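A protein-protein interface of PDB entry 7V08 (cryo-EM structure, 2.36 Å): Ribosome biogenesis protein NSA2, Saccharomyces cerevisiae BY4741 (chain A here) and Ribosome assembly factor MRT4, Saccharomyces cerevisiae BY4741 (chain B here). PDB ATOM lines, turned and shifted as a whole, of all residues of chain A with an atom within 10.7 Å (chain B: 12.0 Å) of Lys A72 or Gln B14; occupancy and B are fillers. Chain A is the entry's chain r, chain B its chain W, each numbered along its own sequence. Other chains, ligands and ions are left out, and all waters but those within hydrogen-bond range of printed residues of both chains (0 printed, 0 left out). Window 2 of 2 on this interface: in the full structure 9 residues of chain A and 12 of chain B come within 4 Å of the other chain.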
ATOM      1  N   LYS A  64     -14.112 -16.361 -10.200  1.00  0.00           N
ATOM      2  CA  LYS A  64     -13.779 -16.810 -11.550  1.00  0.00           C
ATOM      3  C   LYS A  64     -14.935 -16.581 -12.526  1.00  0.00           C
ATOM      4  O   LYS A  64     -14.715 -16.165 -13.673  1.00  0.00           O
ATOM      5  CB  LYS A  64     -13.368 -18.280 -11.538  1.00  0.00           C
ATOM      6  CG  LYS A  64     -12.930 -18.790 -12.895  1.00  0.00           C
ATOM      7  CD  LYS A  64     -12.495 -20.245 -12.860  1.00  0.00           C
ATOM      8  CE  LYS A  64     -11.238 -20.426 -12.045  1.00  0.00           C
ATOM      9  NZ  LYS A  64     -10.769 -21.838 -12.075  1.00  0.00           N
ATOM     10  N   ILE A  65     -16.171 -16.841 -12.092  1.00  0.00           N
ATOM     11  CA  ILE A  65     -17.330 -16.594 -12.952  1.00  0.00           C
ATOM     12  C   ILE A  65     -17.445 -15.109 -13.280  1.00  0.00           C
ATOM     13  O   ILE A  65     -17.697 -14.725 -14.434  1.00  0.00           O
ATOM     14  CB  ILE A  65     -18.620 -17.120 -12.292  1.00  0.00           C
ATOM     15  CG1 ILE A  65     -18.522 -18.617 -11.994  1.00  0.00           C
ATOM     16  CG2 ILE A  65     -19.824 -16.837 -13.165  1.00  0.00           C
ATOM     17  CD1 ILE A  65     -18.373 -19.489 -13.216  1.00  0.00           C
ATOM     18  N   LYS A  66     -17.259 -14.251 -12.270  1.00  0.00           N
ATOM     19  CA  LYS A  66     -17.335 -12.812 -12.491  1.00  0.00           C
ATOM     20  C   LYS A  66     -16.266 -12.340 -13.471  1.00  0.00           C
ATOM     21  O   LYS A  66     -16.545 -11.522 -14.357  1.00  0.00           O
ATOM     22  CB  LYS A  66     -17.202 -12.077 -11.157  1.00  0.00           C
ATOM     23  CG  LYS A  66     -17.427 -10.584 -11.230  1.00  0.00           C
ATOM     24  CD  LYS A  66     -18.852 -10.264 -11.639  1.00  0.00           C
ATOM     25  CE  LYS A  66     -19.084  -8.764 -11.707  1.00  0.00           C
ATOM     26  NZ  LYS A  66     -20.512  -8.426 -11.968  1.00  0.00           N
ATOM     27  N   ALA A  67     -15.039 -12.849 -13.331  1.00  0.00           N
ATOM     28  CA  ALA A  67     -13.968 -12.450 -14.239  1.00  0.00           C
ATOM     29  C   ALA A  67     -14.245 -12.909 -15.662  1.00  0.00           C
ATOM     30  O   ALA A  67     -13.976 -12.176 -16.621  1.00  0.00           O
ATOM     31  CB  ALA A  67     -12.629 -12.999 -13.753  1.00  0.00           C
ATOM     32  N   HIS A  68     -14.778 -14.124 -15.820  1.00  0.00           N
ATOM     33  CA  HIS A  68     -15.101 -14.614 -17.155  1.00  0.00           C
ATOM     34  C   HIS A  68     -16.158 -13.748 -17.824  1.00  0.00           C
ATOM     35  O   HIS A  68     -16.011 -13.376 -18.993  1.00  0.00           O
ATOM     36  CB  HIS A  68     -15.569 -16.064 -17.089  1.00  0.00           C
ATOM     37  CG  HIS A  68     -16.084 -16.590 -18.390  1.00  0.00           C
ATOM     38  ND1 HIS A  68     -15.254 -17.062 -19.382  1.00  0.00           N
ATOM     39  CD2 HIS A  68     -17.346 -16.711 -18.866  1.00  0.00           C
ATOM     40  CE1 HIS A  68     -15.982 -17.458 -20.411  1.00  0.00           C
ATOM     41  NE2 HIS A  68     -17.255 -17.259 -20.121  1.00  0.00           N
ATOM     42  N   GLU A  69     -17.229 -13.408 -17.100  1.00  0.00           N
ATOM     43  CA  GLU A  69     -18.280 -12.597 -17.711  1.00  0.00           C
ATOM     44  C   GLU A  69     -17.796 -11.179 -17.996  1.00  0.00           C
ATOM     45  O   GLU A  69     -18.186 -10.573 -19.002  1.00  0.00           O
ATOM     46  CB  GLU A  69     -19.524 -12.581 -16.829  1.00  0.00           C
ATOM     47  CG  GLU A  69     -20.132 -13.958 -16.631  1.00  0.00           C
ATOM     48  CD  GLU A  69     -20.444 -14.654 -17.945  1.00  0.00           C
ATOM     49  OE1 GLU A  69     -20.941 -13.992 -18.878  1.00  0.00           O
ATOM     50  OE2 GLU A  69     -20.189 -15.867 -18.042  1.00  0.00           O
ATOM     51  N   GLN A  70     -16.936 -10.638 -17.127  1.00  0.00           N
ATOM     52  CA  GLN A  70     -16.360  -9.321 -17.378  1.00  0.00           C
ATOM     53  C   GLN A  70     -15.489  -9.329 -18.627  1.00  0.00           C
ATOM     54  O   GLN A  70     -15.500  -8.369 -19.407  1.00  0.00           O
ATOM     55  CB  GLN A  70     -15.546  -8.873 -16.167  1.00  0.00           C
ATOM     56  CG  GLN A  70     -15.481  -7.377 -15.972  1.00  0.00           C
ATOM     57  CD  GLN A  70     -14.729  -6.992 -14.716  1.00  0.00           C
ATOM     58  OE1 GLN A  70     -14.392  -7.844 -13.896  1.00  0.00           O
ATOM     59  NE2 GLN A  70     -14.456  -5.702 -14.563  1.00  0.00           N
ATOM     60  N   SER A  71     -14.720 -10.400 -18.830  1.00  0.00           N
ATOM     61  CA  SER A  71     -13.906 -10.508 -20.036  1.00  0.00           C
ATOM     62  C   SER A  71     -14.767 -10.682 -21.280  1.00  0.00           C
ATOM     63  O   SER A  71     -14.459 -10.123 -22.339  1.00  0.00           O
ATOM     64  CB  SER A  71     -12.926 -11.671 -19.908  1.00  0.00           C
ATOM     65  OG  SER A  71     -12.138 -11.790 -21.076  1.00  0.00           O
ATOM     66  N   LYS A  72     -15.840 -11.466 -21.178  1.00  0.00           N
ATOM     67  CA  LYS A  72     -16.694 -11.714 -22.332  1.00  0.00           C
ATOM     68  C   LYS A  72     -17.519 -10.498 -22.724  1.00  0.00           C
ATOM     69  O   LYS A  72     -17.863 -10.355 -23.902  1.00  0.00           O
ATOM     70  CB  LYS A  72     -17.623 -12.899 -22.059  1.00  0.00           C
ATOM     71  CG  LYS A  72     -18.111 -13.587 -23.309  1.00  0.00           C
ATOM     72  CD  LYS A  72     -18.375 -15.050 -23.058  1.00  0.00           C
ATOM     73  CE  LYS A  72     -19.580 -15.259 -22.163  1.00  0.00           C
ATOM     74  NZ  LYS A  72     -19.744 -16.699 -21.840  1.00  0.00           N
ATOM     75  N   VAL A  73     -17.849  -9.630 -21.764  1.00  0.00           N
ATOM     76  CA  VAL A  73     -18.489  -8.361 -22.102  1.00  0.00           C
ATOM     77  C   VAL A  73     -17.578  -7.539 -23.004  1.00  0.00           C
ATOM     78  O   VAL A  73     -18.021  -6.976 -24.012  1.00  0.00           O
ATOM     79  CB  VAL A  73     -18.866  -7.595 -20.820  1.00  0.00           C
ATOM     80  CG1 VAL A  73     -19.021  -6.112 -21.103  1.00  0.00           C
ATOM     81  CG2 VAL A  73     -20.145  -8.154 -20.230  1.00  0.00           C
ATOM     82  N   LYS A  74     -16.293  -7.478 -22.667  1.00  0.00           N
ATOM     83  CA  LYS A  74     -15.304  -6.765 -23.463  1.00  0.00           C
ATOM     84  C   LYS A  74     -14.437  -7.727 -24.265  1.00  0.00           C
ATOM     85  O   LYS A  74     -13.245  -7.879 -23.993  1.00  0.00           O
ATOM     86  CB  LYS A  74     -14.416  -5.903 -22.567  1.00  0.00           C
ATOM     87  CG  LYS A  74     -15.135  -4.747 -21.895  1.00  0.00           C
ATOM     88  CD  LYS A  74     -14.208  -4.063 -20.909  1.00  0.00           C
ATOM     89  CE  LYS A  74     -14.822  -2.801 -20.338  1.00  0.00           C
ATOM     90  NZ  LYS A  74     -13.920  -2.165 -19.341  1.00  0.00           N
ATOM     91  N   LEU B   9     -23.746 -28.423 -14.472  1.00  0.00           N
ATOM     92  CA  LEU B   9     -22.367 -28.092 -14.802  1.00  0.00           C
ATOM     93  C   LEU B   9     -22.272 -26.675 -15.349  1.00  0.00           C
ATOM     94  O   LEU B   9     -23.123 -26.233 -16.126  1.00  0.00           O
ATOM     95  CB  LEU B   9     -21.810 -29.077 -15.825  1.00  0.00           C
ATOM     96  CG  LEU B   9     -21.920 -30.564 -15.498  1.00  0.00           C
ATOM     97  CD1 LEU B   9     -21.159 -31.389 -16.533  1.00  0.00           C
ATOM     98  CD2 LEU B   9     -21.408 -30.841 -14.095  1.00  0.00           C
ATOM     99  N   VAL B  10     -21.219 -25.966 -14.950  1.00  0.00           N
ATOM    100  CA  VAL B  10     -20.967 -24.601 -15.394  1.00  0.00           C
ATOM    101  C   VAL B  10     -19.742 -24.606 -16.296  1.00  0.00           C
ATOM    102  O   VAL B  10     -18.678 -25.105 -15.909  1.00  0.00           O
ATOM    103  CB  VAL B  10     -20.767 -23.643 -14.206  1.00  0.00           C
ATOM    104  CG1 VAL B  10     -20.634 -22.212 -14.702  1.00  0.00           C
ATOM    105  CG2 VAL B  10     -21.922 -23.766 -13.227  1.00  0.00           C
ATOM    106  N   THR B  11     -19.892 -24.054 -17.495  1.00  0.00           N
ATOM    107  CA  THR B  11     -18.805 -23.939 -18.454  1.00  0.00           C
ATOM    108  C   THR B  11     -18.525 -22.469 -18.720  1.00  0.00           C
ATOM    109  O   THR B  11     -19.440 -21.639 -18.708  1.00  0.00           O
ATOM    110  CB  THR B  11     -19.133 -24.634 -19.774  1.00  0.00           C
ATOM    111  OG1 THR B  11     -20.098 -23.853 -20.489  1.00  0.00           O
ATOM    112  CG2 THR B  11     -19.700 -26.018 -19.523  1.00  0.00           C
ATOM    113  N   LEU B  12     -17.259 -22.152 -18.960  1.00  0.00           N
ATOM    114  CA  LEU B  12     -16.839 -20.790 -19.270  1.00  0.00           C
ATOM    115  C   LEU B  12     -16.389 -20.774 -20.726  1.00  0.00           C
ATOM    116  O   LEU B  12     -15.206 -20.889 -21.032  1.00  0.00           O
ATOM    117  CB  LEU B  12     -15.738 -20.338 -18.320  1.00  0.00           C
ATOM    118  CG  LEU B  12     -16.163 -20.296 -16.854  1.00  0.00           C
ATOM    119  CD1 LEU B  12     -15.039 -19.774 -15.971  1.00  0.00           C
ATOM    120  CD2 LEU B  12     -17.401 -19.441 -16.706  1.00  0.00           C
ATOM    121  N   ALA B  13     -17.350 -20.621 -21.629  1.00  0.00           N
ATOM    122  CA  ALA B  13     -17.082 -20.570 -23.054  1.00  0.00           C
ATOM    123  C   ALA B  13     -17.408 -19.175 -23.580  1.00  0.00           C
ATOM    124  O   ALA B  13     -17.896 -18.313 -22.846  1.00  0.00           O
ATOM    125  CB  ALA B  13     -17.873 -21.661 -23.779  1.00  0.00           C
ATOM    126  N   GLN B  14     -17.146 -18.957 -24.868  1.00  0.00           N
ATOM    127  CA  GLN B  14     -17.266 -17.631 -25.460  1.00  0.00           C
ATOM    128  C   GLN B  14     -18.555 -17.424 -26.243  1.00  0.00           C
ATOM    129  O   GLN B  14     -18.758 -16.334 -26.787  1.00  0.00           O
ATOM    130  CB  GLN B  14     -16.070 -17.349 -26.380  1.00  0.00           C
ATOM    131  CG  GLN B  14     -14.730 -17.230 -25.660  1.00  0.00           C
ATOM    132  CD  GLN B  14     -14.593 -15.929 -24.893  1.00  0.00           C
ATOM    133  OE1 GLN B  14     -15.347 -14.985 -25.117  1.00  0.00           O
ATOM    134  NE2 GLN B  14     -13.621 -15.871 -23.988  1.00  0.00           N
ATOM    135  N   THR B  15     -19.425 -18.424 -26.312  1.00  0.00           N
ATOM    136  CA  THR B  15     -20.649 -18.346 -27.097  1.00  0.00           C
ATOM    137  C   THR B  15     -21.863 -18.498 -26.188  1.00  0.00           C
ATOM    138  O   THR B  15     -21.901 -19.397 -25.342  1.00  0.00           O
ATOM    139  CB  THR B  15     -20.661 -19.423 -28.184  1.00  0.00           C
ATOM    140  OG1 THR B  15     -19.482 -19.302 -28.982  1.00  0.00           O
ATOM    141  CG2 THR B  15     -21.873 -19.273 -29.075  1.00  0.00           C
ATOM    142  N   ASP B  16     -22.846 -17.620 -26.368  1.00  0.00           N
ATOM    143  CA  ASP B  16     -24.118 -17.671 -25.662  1.00  0.00           C
ATOM    144  C   ASP B  16     -25.180 -18.340 -26.529  1.00  0.00           C
ATOM    145  O   ASP B  16     -24.964 -18.627 -27.708  1.00  0.00           O
ATOM    146  CB  ASP B  16     -24.580 -16.266 -25.264  1.00  0.00           C
ATOM    147  CG  ASP B  16     -23.713 -15.647 -24.183  1.00  0.00           C
ATOM    148  OD1 ASP B  16     -22.579 -16.126 -23.972  1.00  0.00           O
ATOM    149  OD2 ASP B  16     -24.173 -14.684 -23.532  1.00  0.00           O
ATOM    150  N   LYS B  17     -26.337 -18.593 -25.923  1.00  0.00           N
ATOM    151  CA  LYS B  17     -27.431 -19.241 -26.628  1.00  0.00           C
ATOM    152  C   LYS B  17     -28.264 -18.231 -27.407  1.00  0.00           C
ATOM    153  O   LYS B  17     -28.243 -17.029 -27.136  1.00  0.00           O
ATOM    154  CB  LYS B  17     -28.320 -20.005 -25.648  1.00  0.00           C
ATOM    155  CG  LYS B  17     -27.753 -21.356 -25.250  1.00  0.00           C
ATOM    156  CD  LYS B  17     -28.676 -22.139 -24.338  1.00  0.00           C
ATOM    157  CE  LYS B  17     -28.056 -23.489 -24.013  1.00  0.00           C
ATOM    158  NZ  LYS B  17     -28.889 -24.328 -23.116  1.00  0.00           N
ATOM    159  N   LYS B  18     -28.997 -18.737 -28.394  1.00  0.00           N
ATOM    160  CA  LYS B  18     -29.895 -17.913 -29.191  1.00  0.00           C
ATOM    161  C   LYS B  18     -31.281 -17.889 -28.559  1.00  0.00           C
ATOM    162  O   LYS B  18     -31.764 -18.907 -28.053  1.00  0.00           O
ATOM    163  CB  LYS B  18     -29.982 -18.441 -30.626  1.00  0.00           C
ATOM    164  CG  LYS B  18     -28.929 -17.887 -31.584  1.00  0.00           C
ATOM    165  CD  LYS B  18     -27.523 -18.349 -31.230  1.00  0.00           C
ATOM    166  CE  LYS B  18     -26.460 -17.494 -31.911  1.00  0.00           C
ATOM    167  NZ  LYS B  18     -25.069 -17.905 -31.545  1.00  0.00           N
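The backbone carbonyl oxygen (O) of Ala B13 lies within hydrogen-bond range of a ring nitrogen (NE2) of His A68 (3.0 Å).
O of Ala B13 lies within hydrogen-bond range of NZ of Lys A72 (2.7 Å).
The side-chain carboxylate (OD1) of Asp B16 is in salt-bridge range of the side-chain amino group (NZ) of Lys A72, at 3.6 Å.
A ring nitrogen (NE2) of His A68 is in hydrogen-bond range of the side-chain amino group (NZ) of Lys A72 (3.1 Å).
NZ of Lys A72 is in salt-bridge range of OE2 of Glu A69 (3.9 Å).
Among the printed residues, pairs that only touch across the chains: Lys A64 with Leu B12, Ile A65 with Val B10, Ile A65 with Leu B12, His A68 with Leu B12 and Lys A72 with Gln B14.
Of the printed residues of chain B, Lys A64 touches Leu B12 (3.9 Å).
Of the printed residues of chain B, Ile A65 touches Val B10 (3.8 Å) and Leu B12 (3.6 Å).
His A68 touches just these residues of chain B: Leu B12 (3.4 Å) and Ala B13 (3.0 Å).
No residue of chain B comes within 4 Å of Glu A69.
No residue of chain B comes within 4 Å of Ser A71.
Lys A72 touches three residues of chain B.
No residue of chain B comes within 4 Å of Val A73.
Printed residues of chain A within 4 Å of Leu B12: Lys A64 (3.9 Å), Ile A65 (3.6 Å) and His A68 (3.4 Å).
Ala B13 touches just these residues of chain A: His A68 and Lys A72.
Printed residues of chain A within 4 Å of Gln B14: Lys A72.
No residue of chain A comes within 4 Å of Thr B15.
Printed residues of chain A within 4 Å of Asp B16: Lys A72 (3.6 Å).
The nearest residue of chain B that does not touch Lys A72 is Thr B15 (4.8 Å).
The nearest residue of chain A that does not touch Gln B14 is His A68 (4.6 Å).
Printed residues of chain A that touch a printed residue of chain B: Lys A64, Ile A65, His A68 and Lys A72.
Hydrophobic or aromatic side chains of chain A within 4 Å of the printed part of chain B: Ile A65 and His A68.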
